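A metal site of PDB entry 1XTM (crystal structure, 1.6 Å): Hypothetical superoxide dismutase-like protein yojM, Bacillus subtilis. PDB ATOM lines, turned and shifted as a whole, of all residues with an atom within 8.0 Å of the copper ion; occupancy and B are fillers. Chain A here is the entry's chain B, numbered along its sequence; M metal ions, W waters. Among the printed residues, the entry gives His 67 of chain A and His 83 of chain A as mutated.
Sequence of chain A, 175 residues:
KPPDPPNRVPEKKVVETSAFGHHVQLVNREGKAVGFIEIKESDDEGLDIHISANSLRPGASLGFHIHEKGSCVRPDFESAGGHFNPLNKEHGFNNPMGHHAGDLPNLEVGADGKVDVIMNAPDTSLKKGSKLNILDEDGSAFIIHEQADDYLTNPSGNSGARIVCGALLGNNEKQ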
ATOM      1  N   GLY A  63      23.803   6.392  -6.076  1.00  0.00           N
ATOM      2  CA  GLY A  63      22.536   5.670  -5.971  1.00  0.00           C
ATOM      3  C   GLY A  63      22.736   4.317  -5.316  1.00  0.00           C
ATOM      4  O   GLY A  63      23.725   3.599  -5.565  1.00  0.00           O
ATOM      5  N   PHE A  64      21.759   3.917  -4.523  1.00  0.00           N
ATOM      6  CA  PHE A  64      21.898   2.746  -3.708  1.00  0.00           C
ATOM      7  C   PHE A  64      20.521   2.131  -3.486  1.00  0.00           C
ATOM      8  O   PHE A  64      19.631   2.779  -2.917  1.00  0.00           O
ATOM      9  CB  PHE A  64      22.476   3.128  -2.351  1.00  0.00           C
ATOM     10  CG  PHE A  64      22.754   1.942  -1.444  1.00  0.00           C
ATOM     11  CD1 PHE A  64      23.309   0.730  -1.962  1.00  0.00           C
ATOM     12  CD2 PHE A  64      22.599   2.078  -0.037  1.00  0.00           C
ATOM     13  CE1 PHE A  64      23.595  -0.329  -1.089  1.00  0.00           C
ATOM     14  CE2 PHE A  64      22.916   1.013   0.835  1.00  0.00           C
ATOM     15  CZ  PHE A  64      23.423  -0.193   0.305  1.00  0.00           C
ATOM     16  N   HIS A  65      20.368   0.883  -3.929  1.00  0.00           N
ATOM     17  CA  HIS A  65      19.046   0.223  -3.962  1.00  0.00           C
ATOM     18  C   HIS A  65      19.142  -1.238  -3.678  1.00  0.00           C
ATOM     19  O   HIS A  65      20.153  -1.903  -4.091  1.00  0.00           O
ATOM     20  CB  HIS A  65      18.354   0.300  -5.352  1.00  0.00           C
ATOM     21  CG  HIS A  65      18.483   1.631  -6.039  1.00  0.00           C
ATOM     22  ND1 HIS A  65      18.936   1.748  -7.335  1.00  0.00           N
ATOM     23  CD2 HIS A  65      18.160   2.890  -5.638  1.00  0.00           C
ATOM     24  CE1 HIS A  65      18.926   3.022  -7.689  1.00  0.00           C
ATOM     25  NE2 HIS A  65      18.460   3.735  -6.684  1.00  0.00           N
ATOM     26  N   ILE A  66      18.090  -1.771  -3.076  1.00  0.00           N
ATOM     27  CA  ILE A  66      17.933  -3.213  -2.998  1.00  0.00           C
ATOM     28  C   ILE A  66      17.167  -3.650  -4.235  1.00  0.00           C
ATOM     29  O   ILE A  66      16.043  -3.158  -4.537  1.00  0.00           O
ATOM     30  CB  ILE A  66      17.198  -3.698  -1.705  1.00  0.00           C
ATOM     31  CG1 ILE A  66      17.912  -3.177  -0.456  1.00  0.00           C
ATOM     32  CG2 ILE A  66      17.146  -5.234  -1.686  1.00  0.00           C
ATOM     33  CD1 ILE A  66      17.117  -3.354   0.867  1.00  0.00           C
ATOM     34  N   HIS A  67      17.790  -4.554  -4.997  1.00  0.00           N
ATOM     35  CA  HIS A  67      17.183  -5.097  -6.217  1.00  0.00           C
ATOM     36  C   HIS A  67      16.542  -6.492  -5.935  1.00  0.00           C
ATOM     37  O   HIS A  67      16.886  -7.160  -4.943  1.00  0.00           O
ATOM     38  CB  HIS A  67      18.230  -5.181  -7.343  1.00  0.00           C
ATOM     39  CG  HIS A  67      18.573  -3.845  -7.932  1.00  0.00           C
ATOM     40  ND1 HIS A  67      18.341  -3.542  -9.261  1.00  0.00           N
ATOM     41  CD2 HIS A  67      19.060  -2.712  -7.376  1.00  0.00           C
ATOM     42  CE1 HIS A  67      18.728  -2.304  -9.510  1.00  0.00           C
ATOM     43  NE2 HIS A  67      19.168  -1.781  -8.375  1.00  0.00           N
ATOM     44  N   ALA A  80      20.555  -9.173 -11.400  1.00  0.00           N
ATOM     45  CA  ALA A  80      19.682  -8.587 -10.395  1.00  0.00           C
ATOM     46  C   ALA A  80      18.344  -7.943 -10.561  1.00  0.00           C
ATOM     47  O   ALA A  80      17.595  -8.027  -9.575  1.00  0.00           O
ATOM     48  CB  ALA A  80      20.556  -7.634  -9.462  1.00  0.00           C
ATOM     49  N   GLY A  81      17.922  -7.516 -11.760  1.00  0.00           N
ATOM     50  CA  GLY A  81      16.489  -7.524 -12.169  1.00  0.00           C
ATOM     51  C   GLY A  81      16.220  -6.197 -11.379  1.00  0.00           C
ATOM     52  O   GLY A  81      17.098  -5.323 -11.387  1.00  0.00           O
ATOM     53  N   GLY A  82      15.018  -5.835 -10.932  1.00  0.00           N
ATOM     54  CA  GLY A  82      14.499  -4.484 -11.110  1.00  0.00           C
ATOM     55  C   GLY A  82      14.635  -4.064  -9.603  1.00  0.00           C
ATOM     56  O   GLY A  82      15.087  -4.875  -8.788  1.00  0.00           O
ATOM     57  N   HIS A  83      14.283  -2.840  -9.194  1.00  0.00           N
ATOM     58  CA  HIS A  83      14.278  -2.476  -7.768  1.00  0.00           C
ATOM     59  C   HIS A  83      13.218  -3.317  -7.018  1.00  0.00           C
ATOM     60  O   HIS A  83      12.160  -3.617  -7.598  1.00  0.00           O
ATOM     61  CB  HIS A  83      13.891  -1.001  -7.568  1.00  0.00           C
ATOM     62  CG  HIS A  83      14.877  -0.012  -8.092  1.00  0.00           C
ATOM     63  ND1 HIS A  83      14.754   1.354  -7.891  1.00  0.00           N
ATOM     64  CD2 HIS A  83      16.029  -0.185  -8.798  1.00  0.00           C
ATOM     65  CE1 HIS A  83      15.778   1.973  -8.458  1.00  0.00           C
ATOM     66  NE2 HIS A  83      16.566   1.070  -8.998  1.00  0.00           N
ATOM     67  N   PHE A  84      13.493  -3.689  -5.778  1.00  0.00           N
ATOM     68  CA  PHE A  84      12.604  -4.551  -4.984  1.00  0.00           C
ATOM     69  C   PHE A  84      11.356  -3.696  -4.742  1.00  0.00           C
ATOM     70  O   PHE A  84      11.468  -2.586  -4.205  1.00  0.00           O
ATOM     71  CB  PHE A  84      13.283  -4.924  -3.669  1.00  0.00           C
ATOM     72  CG  PHE A  84      12.403  -5.674  -2.694  1.00  0.00           C
ATOM     73  CD1 PHE A  84      12.244  -5.203  -1.377  1.00  0.00           C
ATOM     74  CD2 PHE A  84      11.808  -6.875  -3.043  1.00  0.00           C
ATOM     75  CE1 PHE A  84      11.459  -5.916  -0.441  1.00  0.00           C
ATOM     76  CE2 PHE A  84      11.013  -7.585  -2.104  1.00  0.00           C
ATOM     77  CZ  PHE A  84      10.859  -7.086  -0.793  1.00  0.00           C
ATOM     78  N   HIS A  91       9.306   4.801  -8.722  1.00  0.00           N
ATOM     79  CA  HIS A  91      10.542   5.116  -8.028  1.00  0.00           C
ATOM     80  C   HIS A  91      10.532   6.475  -7.311  1.00  0.00           C
ATOM     81  O   HIS A  91      10.039   7.461  -7.841  1.00  0.00           O
ATOM     82  CB  HIS A  91      11.726   5.052  -9.011  1.00  0.00           C
ATOM     83  CG  HIS A  91      13.033   5.393  -8.377  1.00  0.00           C
ATOM     84  ND1 HIS A  91      13.716   4.503  -7.550  1.00  0.00           N
ATOM     85  CD2 HIS A  91      13.754   6.537  -8.371  1.00  0.00           C
ATOM     86  CE1 HIS A  91      14.796   5.097  -7.078  1.00  0.00           C
ATOM     87  NE2 HIS A  91      14.858   6.326  -7.573  1.00  0.00           N
ATOM     88  N   GLY A 102      12.657  -1.058  -1.995  1.00  0.00           N
ATOM     89  CA  GLY A 102      14.139  -1.195  -2.149  1.00  0.00           C
ATOM     90  C   GLY A 102      14.876   0.130  -2.298  1.00  0.00           C
ATOM     91  O   GLY A 102      16.131   0.156  -2.456  1.00  0.00           O
ATOM     92  N   ASP A 103      14.160   1.264  -2.250  1.00  0.00           N
ATOM     93  CA  ASP A 103      14.821   2.559  -2.449  1.00  0.00           C
ATOM     94  C   ASP A 103      15.507   2.962  -1.192  1.00  0.00           C
ATOM     95  O   ASP A 103      14.861   3.031  -0.143  1.00  0.00           O
ATOM     96  CB  ASP A 103      13.865   3.700  -2.925  1.00  0.00           C
ATOM     97  CG  ASP A 103      13.375   3.478  -4.335  1.00  0.00           C
ATOM     98  OD1 ASP A 103      12.417   4.167  -4.790  1.00  0.00           O
ATOM     99  OD2 ASP A 103      13.882   2.614  -5.103  1.00  0.00           O
ATOM    100  N   ALA A 141      19.656  -8.247  -4.115  1.00  0.00           N
ATOM    101  CA  ALA A 141      21.047  -7.735  -4.317  1.00  0.00           C
ATOM    102  C   ALA A 141      21.128  -6.271  -3.893  1.00  0.00           C
ATOM    103  O   ALA A 141      20.239  -5.484  -4.227  1.00  0.00           O
ATOM    104  CB  ALA A 141      21.475  -7.871  -5.744  1.00  0.00           C
ATOM    105  N   PHE A 142      22.182  -5.900  -3.187  1.00  0.00           N
ATOM    106  CA  PHE A 142      22.413  -4.502  -2.893  1.00  0.00           C
ATOM    107  C   PHE A 142      23.279  -3.938  -4.014  1.00  0.00           C
ATOM    108  O   PHE A 142      24.338  -4.524  -4.315  1.00  0.00           O
ATOM    109  CB  PHE A 142      23.153  -4.416  -1.572  1.00  0.00           C
ATOM    110  CG  PHE A 142      22.318  -4.860  -0.404  1.00  0.00           C
ATOM    111  CD1 PHE A 142      21.524  -3.922   0.279  1.00  0.00           C
ATOM    112  CD2 PHE A 142      22.274  -6.184  -0.039  1.00  0.00           C
ATOM    113  CE1 PHE A 142      20.740  -4.317   1.381  1.00  0.00           C
ATOM    114  CE2 PHE A 142      21.484  -6.580   1.100  1.00  0.00           C
ATOM    115  CZ  PHE A 142      20.704  -5.616   1.773  1.00  0.00           C
ATOM    116  N   ILE A 143      22.862  -2.852  -4.639  1.00  0.00           N
ATOM    117  CA  ILE A 143      23.590  -2.316  -5.801  1.00  0.00           C
ATOM    118  C   ILE A 143      23.928  -0.841  -5.591  1.00  0.00           C
ATOM    119  O   ILE A 143      23.051  -0.047  -5.239  1.00  0.00           O
ATOM    120  CB  ILE A 143      22.813  -2.568  -7.103  1.00  0.00           C
ATOM    121  CG1 ILE A 143      22.620  -4.070  -7.323  1.00  0.00           C
ATOM    122  CG2 ILE A 143      23.469  -1.870  -8.299  1.00  0.00           C
ATOM    123  CD1 ILE A 143      22.131  -4.490  -8.684  1.00  0.00           C
ATOM    124  N   ILE A 144      25.185  -0.502  -5.839  1.00  0.00           N
ATOM    125  CA  ILE A 144      25.629   0.885  -5.846  1.00  0.00           C
ATOM    126  C   ILE A 144      25.795   1.272  -7.321  1.00  0.00           C
ATOM    127  O   ILE A 144      26.311   0.478  -8.138  1.00  0.00           O
ATOM    128  CB  ILE A 144      27.006   1.098  -5.127  1.00  0.00           C
ATOM    129  CG1 ILE A 144      27.022   0.409  -3.740  1.00  0.00           C
ATOM    130  CG2 ILE A 144      27.320   2.620  -5.002  1.00  0.00           C
ATOM    131  CD1 ILE A 144      28.359   0.442  -2.977  1.00  0.00           C
ATOM    132  N   HIS A 145      25.360   2.479  -7.653  1.00  0.00           N
ATOM    133  CA  HIS A 145      25.358   2.982  -9.020  1.00  0.00           C
ATOM    134  C   HIS A 145      26.435   4.065  -9.243  1.00  0.00           C
ATOM    135  O   HIS A 145      27.032   4.633  -8.290  1.00  0.00           O
ATOM    136  CB  HIS A 145      23.970   3.583  -9.324  1.00  0.00           C
ATOM    137  CG  HIS A 145      22.893   2.548  -9.488  1.00  0.00           C
ATOM    138  ND1 HIS A 145      22.486   2.110 -10.729  1.00  0.00           N
ATOM    139  CD2 HIS A 145      22.135   1.856  -8.580  1.00  0.00           C
ATOM    140  CE1 HIS A 145      21.524   1.208 -10.588  1.00  0.00           C
ATOM    141  NE2 HIS A 145      21.283   1.052  -9.299  1.00  0.00           N
ATOM    142  N   ASP A 149      21.083   9.091  -7.280  1.00  0.00           N
ATOM    143  CA  ASP A 149      19.661   8.882  -7.464  1.00  0.00           C
ATOM    144  C   ASP A 149      18.966  10.265  -7.216  1.00  0.00           C
ATOM    145  O   ASP A 149      19.221  10.900  -6.187  1.00  0.00           O
ATOM    146  CB  ASP A 149      19.206   7.831  -6.437  1.00  0.00           C
ATOM    147  CG  ASP A 149      17.763   7.348  -6.650  1.00  0.00           C
ATOM    148  OD1 ASP A 149      16.919   8.124  -7.183  1.00  0.00           O
ATOM    149  OD2 ASP A 149      17.422   6.197  -6.301  1.00  0.00           O
ATOM    150  N   PRO A 155      12.814   4.496 -14.048  1.00  0.00           N
ATOM    151  CA  PRO A 155      12.469   3.665 -12.881  1.00  0.00           C
ATOM    152  C   PRO A 155      13.585   3.555 -11.813  1.00  0.00           C
ATOM    153  O   PRO A 155      13.389   2.860 -10.804  1.00  0.00           O
ATOM    154  CB  PRO A 155      12.204   2.305 -13.534  1.00  0.00           C
ATOM    155  CG  PRO A 155      13.170   2.270 -14.696  1.00  0.00           C
ATOM    156  CD  PRO A 155      13.503   3.713 -15.093  1.00  0.00           C
ATOM    157  N   SER A 156      14.729   4.211 -12.029  1.00  0.00           N
ATOM    158  CA  SER A 156      15.876   4.134 -11.114  1.00  0.00           C
ATOM    159  C   SER A 156      16.508   5.471 -10.690  1.00  0.00           C
ATOM    160  O   SER A 156      17.646   5.503 -10.222  1.00  0.00           O
ATOM    161  CB  SER A 156      16.960   3.216 -11.716  1.00  0.00           C
ATOM    162  OG  SER A 156      17.017   3.429 -13.126  1.00  0.00           O
ATOM    163  N   GLY A 157      15.782   6.589 -10.859  1.00  0.00           N
ATOM    164  CA  GLY A 157      16.271   7.890 -10.428  1.00  0.00           C
ATOM    165  C   GLY A 157      17.438   8.421 -11.230  1.00  0.00           C
ATOM    166  O   GLY A 157      18.169   9.290 -10.775  1.00  0.00           O
ATOM    167  N   SER A 159      20.119   6.981 -11.896  1.00  0.00           N
ATOM    168  CA  SER A 159      21.325   6.537 -11.181  1.00  0.00           C
ATOM    169  C   SER A 159      22.418   5.989 -12.119  1.00  0.00           C
ATOM    170  O   SER A 159      23.554   5.820 -11.711  1.00  0.00           O
ATOM    171  CB  SER A 159      20.976   5.453 -10.123  1.00  0.00           C
ATOM    172  OG  SER A 159      20.000   5.939  -9.187  1.00  0.00           O
ATOM    173  N   GLY A 160      22.081   5.721 -13.384  1.00  0.00           N
ATOM    174  CA  GLY A 160      23.071   5.179 -14.329  1.00  0.00           C
ATOM    175  C   GLY A 160      23.464   3.748 -14.057  1.00  0.00           C
ATOM    176  O   GLY A 160      22.737   2.961 -13.452  1.00  0.00           O
ATOM    177  N   ALA A 161      24.644   3.392 -14.583  1.00  0.00           N
ATOM    178  CA  ALA A 161      25.161   2.053 -14.495  1.00  0.00           C
ATOM    179  C   ALA A 161      25.289   1.477 -13.077  1.00  0.00           C
ATOM    180  O   ALA A 161      25.541   2.198 -12.082  1.00  0.00           O
ATOM    181  CB  ALA A 161      26.552   1.977 -15.229  1.00  0.00           C
ATOM    182  N   ARG A 162      25.206   0.150 -13.028  1.00  0.00           N
ATOM    183  CA  ARG A 162      25.387  -0.615 -11.810  1.00  0.00           C
ATOM    184  C   ARG A 162      26.883  -0.862 -11.609  1.00  0.00           C
ATOM    185  O   ARG A 162      27.490  -1.505 -12.467  1.00  0.00           O
ATOM    186  CB  ARG A 162      24.619  -1.944 -11.935  1.00  0.00           C
ATOM    187  CG  ARG A 162      23.146  -1.737 -12.109  1.00  0.00           C
ATOM    188  CD  ARG A 162      22.333  -3.010 -12.344  1.00  0.00           C
ATOM    189  NE  ARG A 162      20.941  -2.665 -12.676  1.00  0.00           N
ATOM    190  CZ  ARG A 162      19.906  -3.500 -12.565  1.00  0.00           C
ATOM    191  NH1 ARG A 162      20.066  -4.757 -12.162  1.00  0.00           N
ATOM    192  NH2 ARG A 162      18.690  -3.068 -12.883  1.00  0.00           N
ATOM    193  N   VAL A 164      28.670  -1.757  -8.246  1.00  0.00           N
ATOM    194  CA  VAL A 164      29.050  -2.613  -7.133  1.00  0.00           C
ATOM    195  C   VAL A 164      27.807  -3.421  -6.792  1.00  0.00           C
ATOM    196  O   VAL A 164      26.716  -2.872  -6.772  1.00  0.00           O
ATOM    197  CB  VAL A 164      29.486  -1.826  -5.889  1.00  0.00           C
ATOM    198  CG1 VAL A 164      29.756  -2.792  -4.752  1.00  0.00           C
ATOM    199  CG2 VAL A 164      30.748  -1.016  -6.161  1.00  0.00           C
HETATM  200 CU    CU M   1      19.618   0.232  -8.553  1.00  0.00          CU
HETATM  201 ZN    ZN M   2      13.446   2.538  -7.019  1.00  0.00          ZN
HETATM  202  O   HOH W   1      18.588   0.522 -11.152  1.00  0.00           O
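A ring nitrogen (ND1) of His 145 is in hydrogen-bond range of the backbone carbonyl oxygen (O) of Gly 160, 2.9 Å away. The side-chain carboxylate (OD2) of Asp 149 is in hydrogen-bond range of a ring nitrogen (NE2) of His 65, 2.7 Å away. The backbone carbonyl oxygen (O) of Ala 141 sits at hydrogen-bond distance from the backbone NH (N) of His 67, at 2.7 Å. The backbone carbonyl oxygen of Gly 81 is in hydrogen-bond range of a ring nitrogen (ND1) of His 67, at 3.0 Å. A ring nitrogen (NE2) of His 83 sits close to a ring nitrogen (ND1) of His 65, 3.0 Å away. O of His 65 lies within hydrogen-bond range of N of Ile 143 (2.9 Å). The backbone NH (N) of His 145 sits at hydrogen-bond distance from the backbone carbonyl oxygen (O) of Gly 63, 2.9 Å away. ND1 of His 145 lies close to O of Ala 161.
His 83 touches the copper ion (NE2 to CU, 3.2 Å).
The copper ion is bound by a ring nitrogen (NE2) of His 145 (2.0 Å), a ring nitrogen (ND1) of His 65 (2.1 Å) and a ring nitrogen (NE2) of His 67 (2.1 Å). The copper ion has three donor atoms within binding distance. Slightly farther from the copper ion lies water W1 (2.8 Å).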
